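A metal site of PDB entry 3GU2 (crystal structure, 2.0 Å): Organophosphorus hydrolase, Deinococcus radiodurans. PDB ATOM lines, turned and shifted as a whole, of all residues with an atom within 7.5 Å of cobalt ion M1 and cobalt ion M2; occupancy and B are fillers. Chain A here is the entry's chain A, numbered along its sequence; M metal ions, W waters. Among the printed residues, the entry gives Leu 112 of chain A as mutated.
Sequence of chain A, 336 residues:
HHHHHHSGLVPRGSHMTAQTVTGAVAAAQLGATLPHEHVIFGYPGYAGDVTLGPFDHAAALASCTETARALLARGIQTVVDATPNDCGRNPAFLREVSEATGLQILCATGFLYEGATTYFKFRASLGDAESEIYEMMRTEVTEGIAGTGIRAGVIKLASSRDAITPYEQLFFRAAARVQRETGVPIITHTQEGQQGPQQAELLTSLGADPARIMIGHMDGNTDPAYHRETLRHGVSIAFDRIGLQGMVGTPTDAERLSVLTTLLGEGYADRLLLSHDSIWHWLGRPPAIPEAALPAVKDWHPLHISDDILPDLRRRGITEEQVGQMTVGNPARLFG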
ATOM      1  N   HIS A  36      -2.953 -18.260  22.410  1.00  0.00           N
ATOM      2  CA  HIS A  36      -3.123 -16.831  22.291  1.00  0.00           C
ATOM      3  C   HIS A  36      -4.556 -16.472  21.868  1.00  0.00           C
ATOM      4  O   HIS A  36      -4.906 -16.532  20.691  1.00  0.00           O
ATOM      5  CB  HIS A  36      -2.162 -16.250  21.257  1.00  0.00           C
ATOM      6  CG  HIS A  36      -2.119 -14.759  21.245  1.00  0.00           C
ATOM      7  ND1 HIS A  36      -0.961 -14.032  21.422  1.00  0.00           N
ATOM      8  CD2 HIS A  36      -3.111 -13.838  21.086  1.00  0.00           C
ATOM      9  CE1 HIS A  36      -1.233 -12.737  21.373  1.00  0.00           C
ATOM     10  NE2 HIS A  36      -2.535 -12.590  21.170  1.00  0.00           N
ATOM     11  N   GLU A  37      -5.321 -16.033  22.843  1.00  0.00           N
ATOM     12  CA  GLU A  37      -6.722 -15.674  22.621  1.00  0.00           C
ATOM     13  C   GLU A  37      -7.056 -14.576  23.621  1.00  0.00           C
ATOM     14  O   GLU A  37      -6.314 -14.335  24.573  1.00  0.00           O
ATOM     15  CB  GLU A  37      -7.605 -16.897  22.889  1.00  0.00           C
ATOM     16  CG  GLU A  37      -7.273 -18.168  22.063  1.00  0.00           C
ATOM     17  CD  GLU A  37      -7.494 -17.981  20.567  1.00  0.00           C
ATOM     18  OE1 GLU A  37      -8.411 -17.224  20.180  1.00  0.00           O
ATOM     19  OE2 GLU A  37      -6.786 -18.612  19.751  1.00  0.00           O
ATOM     20  N   HIS A  38      -8.180 -13.886  23.403  1.00  0.00           N
ATOM     21  CA  HIS A  38      -8.583 -12.834  24.340  1.00  0.00           C
ATOM     22  C   HIS A  38     -10.054 -13.066  24.692  1.00  0.00           C
ATOM     23  O   HIS A  38     -10.929 -13.013  23.818  1.00  0.00           O
ATOM     24  CB  HIS A  38      -8.388 -11.464  23.688  1.00  0.00           C
ATOM     25  CG  HIS A  38      -6.985 -11.182  23.233  1.00  0.00           C
ATOM     26  ND1 HIS A  38      -6.002 -10.728  24.090  1.00  0.00           N
ATOM     27  CD2 HIS A  38      -6.391 -11.288  22.013  1.00  0.00           C
ATOM     28  CE1 HIS A  38      -4.873 -10.562  23.423  1.00  0.00           C
ATOM     29  NE2 HIS A  38      -5.087 -10.892  22.164  1.00  0.00           N
ATOM     30  N   PHE A  41     -11.449  -7.938  25.445  1.00  0.00           N
ATOM     31  CA  PHE A  41     -10.333  -7.100  25.009  1.00  0.00           C
ATOM     32  C   PHE A  41     -10.822  -5.717  24.650  1.00  0.00           C
ATOM     33  O   PHE A  41     -11.905  -5.553  24.111  1.00  0.00           O
ATOM     34  CB  PHE A  41      -9.614  -7.734  23.815  1.00  0.00           C
ATOM     35  CG  PHE A  41      -8.483  -6.901  23.269  1.00  0.00           C
ATOM     36  CD1 PHE A  41      -8.730  -5.830  22.421  1.00  0.00           C
ATOM     37  CD2 PHE A  41      -7.162  -7.194  23.600  1.00  0.00           C
ATOM     38  CE1 PHE A  41      -7.680  -5.059  21.891  1.00  0.00           C
ATOM     39  CE2 PHE A  41      -6.099  -6.425  23.075  1.00  0.00           C
ATOM     40  CZ  PHE A  41      -6.367  -5.364  22.222  1.00  0.00           C
ATOM     41  N   ALA A  82      -3.923 -13.806  26.229  1.00  0.00           N
ATOM     42  CA  ALA A  82      -2.784 -12.906  26.060  1.00  0.00           C
ATOM     43  C   ALA A  82      -3.056 -11.405  26.254  1.00  0.00           C
ATOM     44  O   ALA A  82      -2.245 -10.552  25.849  1.00  0.00           O
ATOM     45  CB  ALA A  82      -2.185 -13.129  24.680  1.00  0.00           C
ATOM     46  N   THR A  83      -4.199 -11.069  26.862  1.00  0.00           N
ATOM     47  CA  THR A  83      -4.584  -9.652  27.033  1.00  0.00           C
ATOM     48  C   THR A  83      -3.660  -8.846  27.930  1.00  0.00           C
ATOM     49  O   THR A  83      -3.579  -9.141  29.114  1.00  0.00           O
ATOM     50  CB  THR A  83      -6.011  -9.516  27.623  1.00  0.00           C
ATOM     51  OG1 THR A  83      -6.931 -10.329  26.880  1.00  0.00           O
ATOM     52  CG2 THR A  83      -6.465  -8.044  27.547  1.00  0.00           C
ATOM     53  N   PRO A  84      -2.995  -7.812  27.394  1.00  0.00           N
ATOM     54  CA  PRO A  84      -2.063  -6.936  28.140  1.00  0.00           C
ATOM     55  C   PRO A  84      -2.778  -6.130  29.225  1.00  0.00           C
ATOM     56  O   PRO A  84      -3.976  -5.837  29.112  1.00  0.00           O
ATOM     57  CB  PRO A  84      -1.484  -6.014  27.055  1.00  0.00           C
ATOM     58  CG  PRO A  84      -1.636  -6.850  25.775  1.00  0.00           C
ATOM     59  CD  PRO A  84      -2.992  -7.464  25.964  1.00  0.00           C
ATOM     60  N   LEU A 112       1.175  -3.362  25.852  1.00  0.00           N
ATOM     61  CA  LEU A 112       1.220  -3.318  24.392  1.00  0.00           C
ATOM     62  C   LEU A 112       2.392  -2.405  23.966  1.00  0.00           C
ATOM     63  O   LEU A 112       3.042  -1.792  24.820  1.00  0.00           O
ATOM     64  CB  LEU A 112      -0.098  -2.765  23.844  1.00  0.00           C
ATOM     65  CG  LEU A 112      -0.511  -3.231  22.449  1.00  0.00           C
ATOM     66  CD1 LEU A 112      -0.632  -4.742  22.442  1.00  0.00           C
ATOM     67  CD2 LEU A 112      -1.837  -2.578  22.046  1.00  0.00           C
ATOM     68  N   TYR A 113       2.682  -2.323  22.661  1.00  0.00           N
ATOM     69  CA  TYR A 113       3.781  -1.474  22.156  1.00  0.00           C
ATOM     70  C   TYR A 113       3.609   0.047  22.336  1.00  0.00           C
ATOM     71  O   TYR A 113       2.526   0.526  22.679  1.00  0.00           O
ATOM     72  CB  TYR A 113       4.095  -1.810  20.683  1.00  0.00           C
ATOM     73  CG  TYR A 113       2.875  -2.176  19.840  1.00  0.00           C
ATOM     74  CD1 TYR A 113       2.056  -3.248  20.205  1.00  0.00           C
ATOM     75  CD2 TYR A 113       2.548  -1.446  18.699  1.00  0.00           C
ATOM     76  CE1 TYR A 113       0.929  -3.587  19.455  1.00  0.00           C
ATOM     77  CE2 TYR A 113       1.405  -1.781  17.934  1.00  0.00           C
ATOM     78  CZ  TYR A 113       0.606  -2.850  18.325  1.00  0.00           C
ATOM     79  OH  TYR A 113      -0.523  -3.176  17.602  1.00  0.00           O
ATOM     80  N   KCX A 156       3.664 -11.224  28.628  1.00  0.00           N
ATOM     81  CA  KCX A 156       3.355 -10.864  27.267  1.00  0.00           C
ATOM     82  CB  KCX A 156       1.871 -10.489  27.209  1.00  0.00           C
ATOM     83  CG  KCX A 156       1.477  -9.728  25.959  1.00  0.00           C
ATOM     84  CD  KCX A 156       1.467 -10.592  24.757  1.00  0.00           C
ATOM     85  CE  KCX A 156       0.108 -10.449  24.137  1.00  0.00           C
ATOM     86  NZ  KCX A 156       0.189  -9.944  22.790  1.00  0.00           N
ATOM     87  C   KCX A 156       4.233  -9.678  26.854  1.00  0.00           C
ATOM     88  O   KCX A 156       4.316  -8.680  27.558  1.00  0.00           O
ATOM     89  CX  KCX A 156      -0.874  -9.678  22.036  1.00  0.00           C
ATOM     90  OQ1 KCX A 156      -0.728  -9.263  20.881  1.00  0.00           O
ATOM     91  OQ2 KCX A 156      -2.022  -9.701  22.516  1.00  0.00           O
ATOM     92  N   LEU A 157       4.879  -9.796  25.711  1.00  0.00           N
ATOM     93  CA  LEU A 157       5.735  -8.739  25.203  1.00  0.00           C
ATOM     94  C   LEU A 157       5.302  -8.365  23.808  1.00  0.00           C
ATOM     95  O   LEU A 157       4.772  -9.203  23.083  1.00  0.00           O
ATOM     96  CB  LEU A 157       7.183  -9.224  25.141  1.00  0.00           C
ATOM     97  CG  LEU A 157       7.850  -9.550  26.462  1.00  0.00           C
ATOM     98  CD1 LEU A 157       9.324  -9.909  26.180  1.00  0.00           C
ATOM     99  CD2 LEU A 157       7.752  -8.358  27.413  1.00  0.00           C
ATOM    100  N   ALA A 158       5.561  -7.117  23.418  1.00  0.00           N
ATOM    101  CA  ALA A 158       5.200  -6.635  22.093  1.00  0.00           C
ATOM    102  C   ALA A 158       6.274  -5.696  21.535  1.00  0.00           C
ATOM    103  O   ALA A 158       6.955  -4.993  22.280  1.00  0.00           O
ATOM    104  CB  ALA A 158       3.848  -5.912  22.151  1.00  0.00           C
ATOM    105  N   THR A 188       4.989 -13.498  22.764  1.00  0.00           N
ATOM    106  CA  THR A 188       5.086 -12.165  22.209  1.00  0.00           C
ATOM    107  C   THR A 188       4.089 -11.844  21.106  1.00  0.00           C
ATOM    108  O   THR A 188       3.386 -12.712  20.570  1.00  0.00           O
ATOM    109  CB  THR A 188       6.461 -11.911  21.578  1.00  0.00           C
ATOM    110  OG1 THR A 188       6.493 -12.471  20.258  1.00  0.00           O
ATOM    111  CG2 THR A 188       7.548 -12.544  22.426  1.00  0.00           C
ATOM    112  N   HIS A 189       4.079 -10.574  20.758  1.00  0.00           N
ATOM    113  CA  HIS A 189       3.298 -10.017  19.679  1.00  0.00           C
ATOM    114  C   HIS A 189       4.364  -9.461  18.739  1.00  0.00           C
ATOM    115  O   HIS A 189       5.323  -8.830  19.209  1.00  0.00           O
ATOM    116  CB  HIS A 189       2.416  -8.864  20.218  1.00  0.00           C
ATOM    117  CG  HIS A 189       2.065  -7.825  19.191  1.00  0.00           C
ATOM    118  ND1 HIS A 189       0.826  -7.729  18.607  1.00  0.00           N
ATOM    119  CD2 HIS A 189       2.804  -6.813  18.639  1.00  0.00           C
ATOM    120  CE1 HIS A 189       0.793  -6.717  17.752  1.00  0.00           C
ATOM    121  NE2 HIS A 189       1.989  -6.143  17.755  1.00  0.00           N
ATOM    122  N   THR A 190       4.251  -9.718  17.437  1.00  0.00           N
ATOM    123  CA  THR A 190       5.173  -9.104  16.486  1.00  0.00           C
ATOM    124  C   THR A 190       4.251  -8.288  15.589  1.00  0.00           C
ATOM    125  O   THR A 190       3.126  -8.711  15.297  1.00  0.00           O
ATOM    126  CB  THR A 190       5.956 -10.119  15.601  1.00  0.00           C
ATOM    127  OG1 THR A 190       5.039 -11.003  14.948  1.00  0.00           O
ATOM    128  CG2 THR A 190       6.955 -10.924  16.446  1.00  0.00           C
ATOM    129  N   GLN A 191       4.709  -7.124  15.168  1.00  0.00           N
ATOM    130  CA  GLN A 191       3.904  -6.227  14.336  1.00  0.00           C
ATOM    131  C   GLN A 191       4.139  -6.439  12.855  1.00  0.00           C
ATOM    132  O   GLN A 191       5.280  -6.330  12.369  1.00  0.00           O
ATOM    133  CB  GLN A 191       4.217  -4.774  14.684  1.00  0.00           C
ATOM    134  CG  GLN A 191       3.269  -3.750  14.051  1.00  0.00           C
ATOM    135  CD  GLN A 191       1.834  -3.917  14.532  1.00  0.00           C
ATOM    136  OE1 GLN A 191       1.573  -4.351  15.662  1.00  0.00           O
ATOM    137  NE2 GLN A 191       0.886  -3.555  13.668  1.00  0.00           N
ATOM    138  N   GLY A 216       5.146 -14.620  18.913  1.00  0.00           N
ATOM    139  CA  GLY A 216       3.832 -14.585  18.276  1.00  0.00           C
ATOM    140  C   GLY A 216       3.655 -13.897  16.934  1.00  0.00           C
ATOM    141  O   GLY A 216       4.583 -13.301  16.369  1.00  0.00           O
ATOM    142  N   HIS A 217       2.428 -13.970  16.419  1.00  0.00           N
ATOM    143  CA  HIS A 217       2.036 -13.391  15.147  1.00  0.00           C
ATOM    144  C   HIS A 217       3.025 -13.632  14.024  1.00  0.00           C
ATOM    145  O   HIS A 217       3.209 -12.771  13.156  1.00  0.00           O
ATOM    146  CB  HIS A 217       1.792 -11.888  15.273  1.00  0.00           C
ATOM    147  CG  HIS A 217       0.864 -11.523  16.384  1.00  0.00           C
ATOM    148  ND1 HIS A 217      -0.068 -12.404  16.888  1.00  0.00           N
ATOM    149  CD2 HIS A 217       0.766 -10.410  17.154  1.00  0.00           C
ATOM    150  CE1 HIS A 217      -0.680 -11.868  17.917  1.00  0.00           C
ATOM    151  NE2 HIS A 217      -0.193 -10.655  18.096  1.00  0.00           N
ATOM    152  N   ASP A 240      -0.592 -17.531  15.395  1.00  0.00           N
ATOM    153  CA  ASP A 240      -1.671 -17.271  16.314  1.00  0.00           C
ATOM    154  C   ASP A 240      -2.767 -16.269  15.884  1.00  0.00           C
ATOM    155  O   ASP A 240      -3.509 -15.763  16.723  1.00  0.00           O
ATOM    156  CB  ASP A 240      -1.079 -16.856  17.674  1.00  0.00           C
ATOM    157  CG  ASP A 240      -0.124 -15.658  17.560  1.00  0.00           C
ATOM    158  OD1 ASP A 240      -0.361 -14.819  16.684  1.00  0.00           O
ATOM    159  OD2 ASP A 240       0.843 -15.544  18.356  1.00  0.00           O
ATOM    160  N   ARG A 241      -2.882 -16.005  14.593  1.00  0.00           N
ATOM    161  CA  ARG A 241      -3.928 -15.087  14.140  1.00  0.00           C
ATOM    162  C   ARG A 241      -4.666 -15.732  12.975  1.00  0.00           C
ATOM    163  O   ARG A 241      -5.103 -15.071  12.029  1.00  0.00           O
ATOM    164  CB  ARG A 241      -3.314 -13.749  13.728  1.00  0.00           C
ATOM    165  CG  ARG A 241      -2.522 -13.094  14.838  1.00  0.00           C
ATOM    166  CD  ARG A 241      -2.197 -11.634  14.552  1.00  0.00           C
ATOM    167  NE  ARG A 241      -3.411 -10.832  14.552  1.00  0.00           N
ATOM    168  CZ  ARG A 241      -3.444  -9.508  14.489  1.00  0.00           C
ATOM    169  NH1 ARG A 241      -2.313  -8.822  14.429  1.00  0.00           N
ATOM    170  NH2 ARG A 241      -4.611  -8.876  14.475  1.00  0.00           N
ATOM    171  N   HIS A 276      -5.821 -18.231  17.258  1.00  0.00           N
ATOM    172  CA  HIS A 276      -6.601 -17.308  16.446  1.00  0.00           C
ATOM    173  C   HIS A 276      -6.401 -15.839  16.790  1.00  0.00           C
ATOM    174  O   HIS A 276      -6.486 -14.967  15.904  1.00  0.00           O
ATOM    175  CB  HIS A 276      -8.109 -17.608  16.579  1.00  0.00           C
ATOM    176  CG  HIS A 276      -8.468 -19.062  16.487  1.00  0.00           C
ATOM    177  ND1 HIS A 276      -8.507 -19.894  17.585  1.00  0.00           N
ATOM    178  CD2 HIS A 276      -8.853 -19.827  15.430  1.00  0.00           C
ATOM    179  CE1 HIS A 276      -8.892 -21.103  17.217  1.00  0.00           C
ATOM    180  NE2 HIS A 276      -9.107 -21.093  15.914  1.00  0.00           N
ATOM    181  N   ASP A 277      -6.160 -15.574  18.063  1.00  0.00           N
ATOM    182  CA  ASP A 277      -6.029 -14.199  18.554  1.00  0.00           C
ATOM    183  C   ASP A 277      -7.423 -13.545  18.463  1.00  0.00           C
ATOM    184  O   ASP A 277      -7.559 -12.365  18.141  1.00  0.00           O
ATOM    185  CB  ASP A 277      -5.030 -13.399  17.727  1.00  0.00           C
ATOM    186  CG  ASP A 277      -4.803 -12.024  18.302  1.00  0.00           C
ATOM    187  OD1 ASP A 277      -5.003 -11.884  19.522  1.00  0.00           O
ATOM    188  OD2 ASP A 277      -4.430 -11.109  17.561  1.00  0.00           O
ATOM    189  N   SER A 278      -8.440 -14.330  18.783  1.00  0.00           N
ATOM    190  CA  SER A 278      -9.810 -13.865  18.726  1.00  0.00           C
ATOM    191  C   SER A 278     -10.197 -13.068  19.963  1.00  0.00           C
ATOM    192  O   SER A 278      -9.492 -13.092  20.976  1.00  0.00           O
ATOM    193  CB  SER A 278     -10.736 -15.085  18.585  1.00  0.00           C
ATOM    194  OG  SER A 278     -10.631 -15.911  19.724  1.00  0.00           O
ATOM    195  N   ILE A 279     -11.331 -12.375  19.863  1.00  0.00           N
ATOM    196  CA  ILE A 279     -11.845 -11.598  20.979  1.00  0.00           C
ATOM    197  C   ILE A 279     -13.265 -12.073  21.180  1.00  0.00           C
ATOM    198  O   ILE A 279     -14.106 -11.921  20.298  1.00  0.00           O
ATOM    199  CB  ILE A 279     -11.827 -10.099  20.643  1.00  0.00           C
ATOM    200  CG1 ILE A 279     -10.361  -9.639  20.530  1.00  0.00           C
ATOM    201  CG2 ILE A 279     -12.608  -9.304  21.720  1.00  0.00           C
ATOM    202  CD1 ILE A 279     -10.162  -8.250  20.016  1.00  0.00           C
HETATM  203 CO    CO M   1      -3.553 -10.641  20.822  1.00  0.00          CO
HETATM  204 CO    CO M   2      -1.133  -8.858  19.168  1.00  0.00          CO
HETATM  205  O   HOH W   1      -1.801  -8.139  16.895  1.00  0.00           O
HETATM  206  O   HOH W   2      -2.223  -6.921  19.817  1.00  0.00           O
HETATM  207  O   HOH W   3      -4.497  -8.882  18.572  1.00  0.00           O
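Cobalt ion M1 is bound by NE2 of His 38 (2.1 Å), NE2 of His 36 (2.2 Å), OD1 of Asp 277 (2.3 Å) and OQ2 of KCX 156 (2.5 Å). Cobalt ion M1 has four donor atoms within binding distance.
Within 4 Å of cobalt ion M2: KCX 156, His 189 and His 217. Along chain A the residues within 4 Å of cobalt ion M2 span positions 156 to 217. The nearest printed residue that does not touch cobalt ion M2 is Asp 277 (4.3 Å).
Within 4 Å of cobalt ion M1: His 36, His 38, KCX 156 and Asp 277.
Cobalt ion M2 is bound by OQ1 of KCX 156 (1.8 Å). NE2 of His 217 binds cobalt ion M2 (2.3 Å). Water W2 binds cobalt ion M2, at 2.3 Å. Cobalt ion M2 is bound by ND1 of His 189 (2.3 Å). Water W1 binds cobalt ion M2 (2.5 Å).
OD2 of Asp 277 is in salt-bridge range of NE of Arg 241 (3.2 Å). N of Asp 277 sits at hydrogen-bond distance from O of Asp 240, at 3.0 Å. The backbone NH of His 189 lies within hydrogen-bond range of the backbone carbonyl oxygen of Leu 157, at 2.8 Å. The side-chain carboxylate (OD1) of Asp 240 lies within hydrogen-bond range of a ring nitrogen (ND1) of His 217. O of His 217 sits at hydrogen-bond distance from OG1 of Thr 190 (3.1 Å). A ring nitrogen (NE2) of His 189 lies within hydrogen-bond range of the side-chain amide oxygen (OE1) of Gln 191. O of Ser 278 lies within hydrogen-bond range of N of His 38. ND1 of His 38 sits at hydrogen-bond distance from OG1 of Thr 83, 3.0 Å away.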
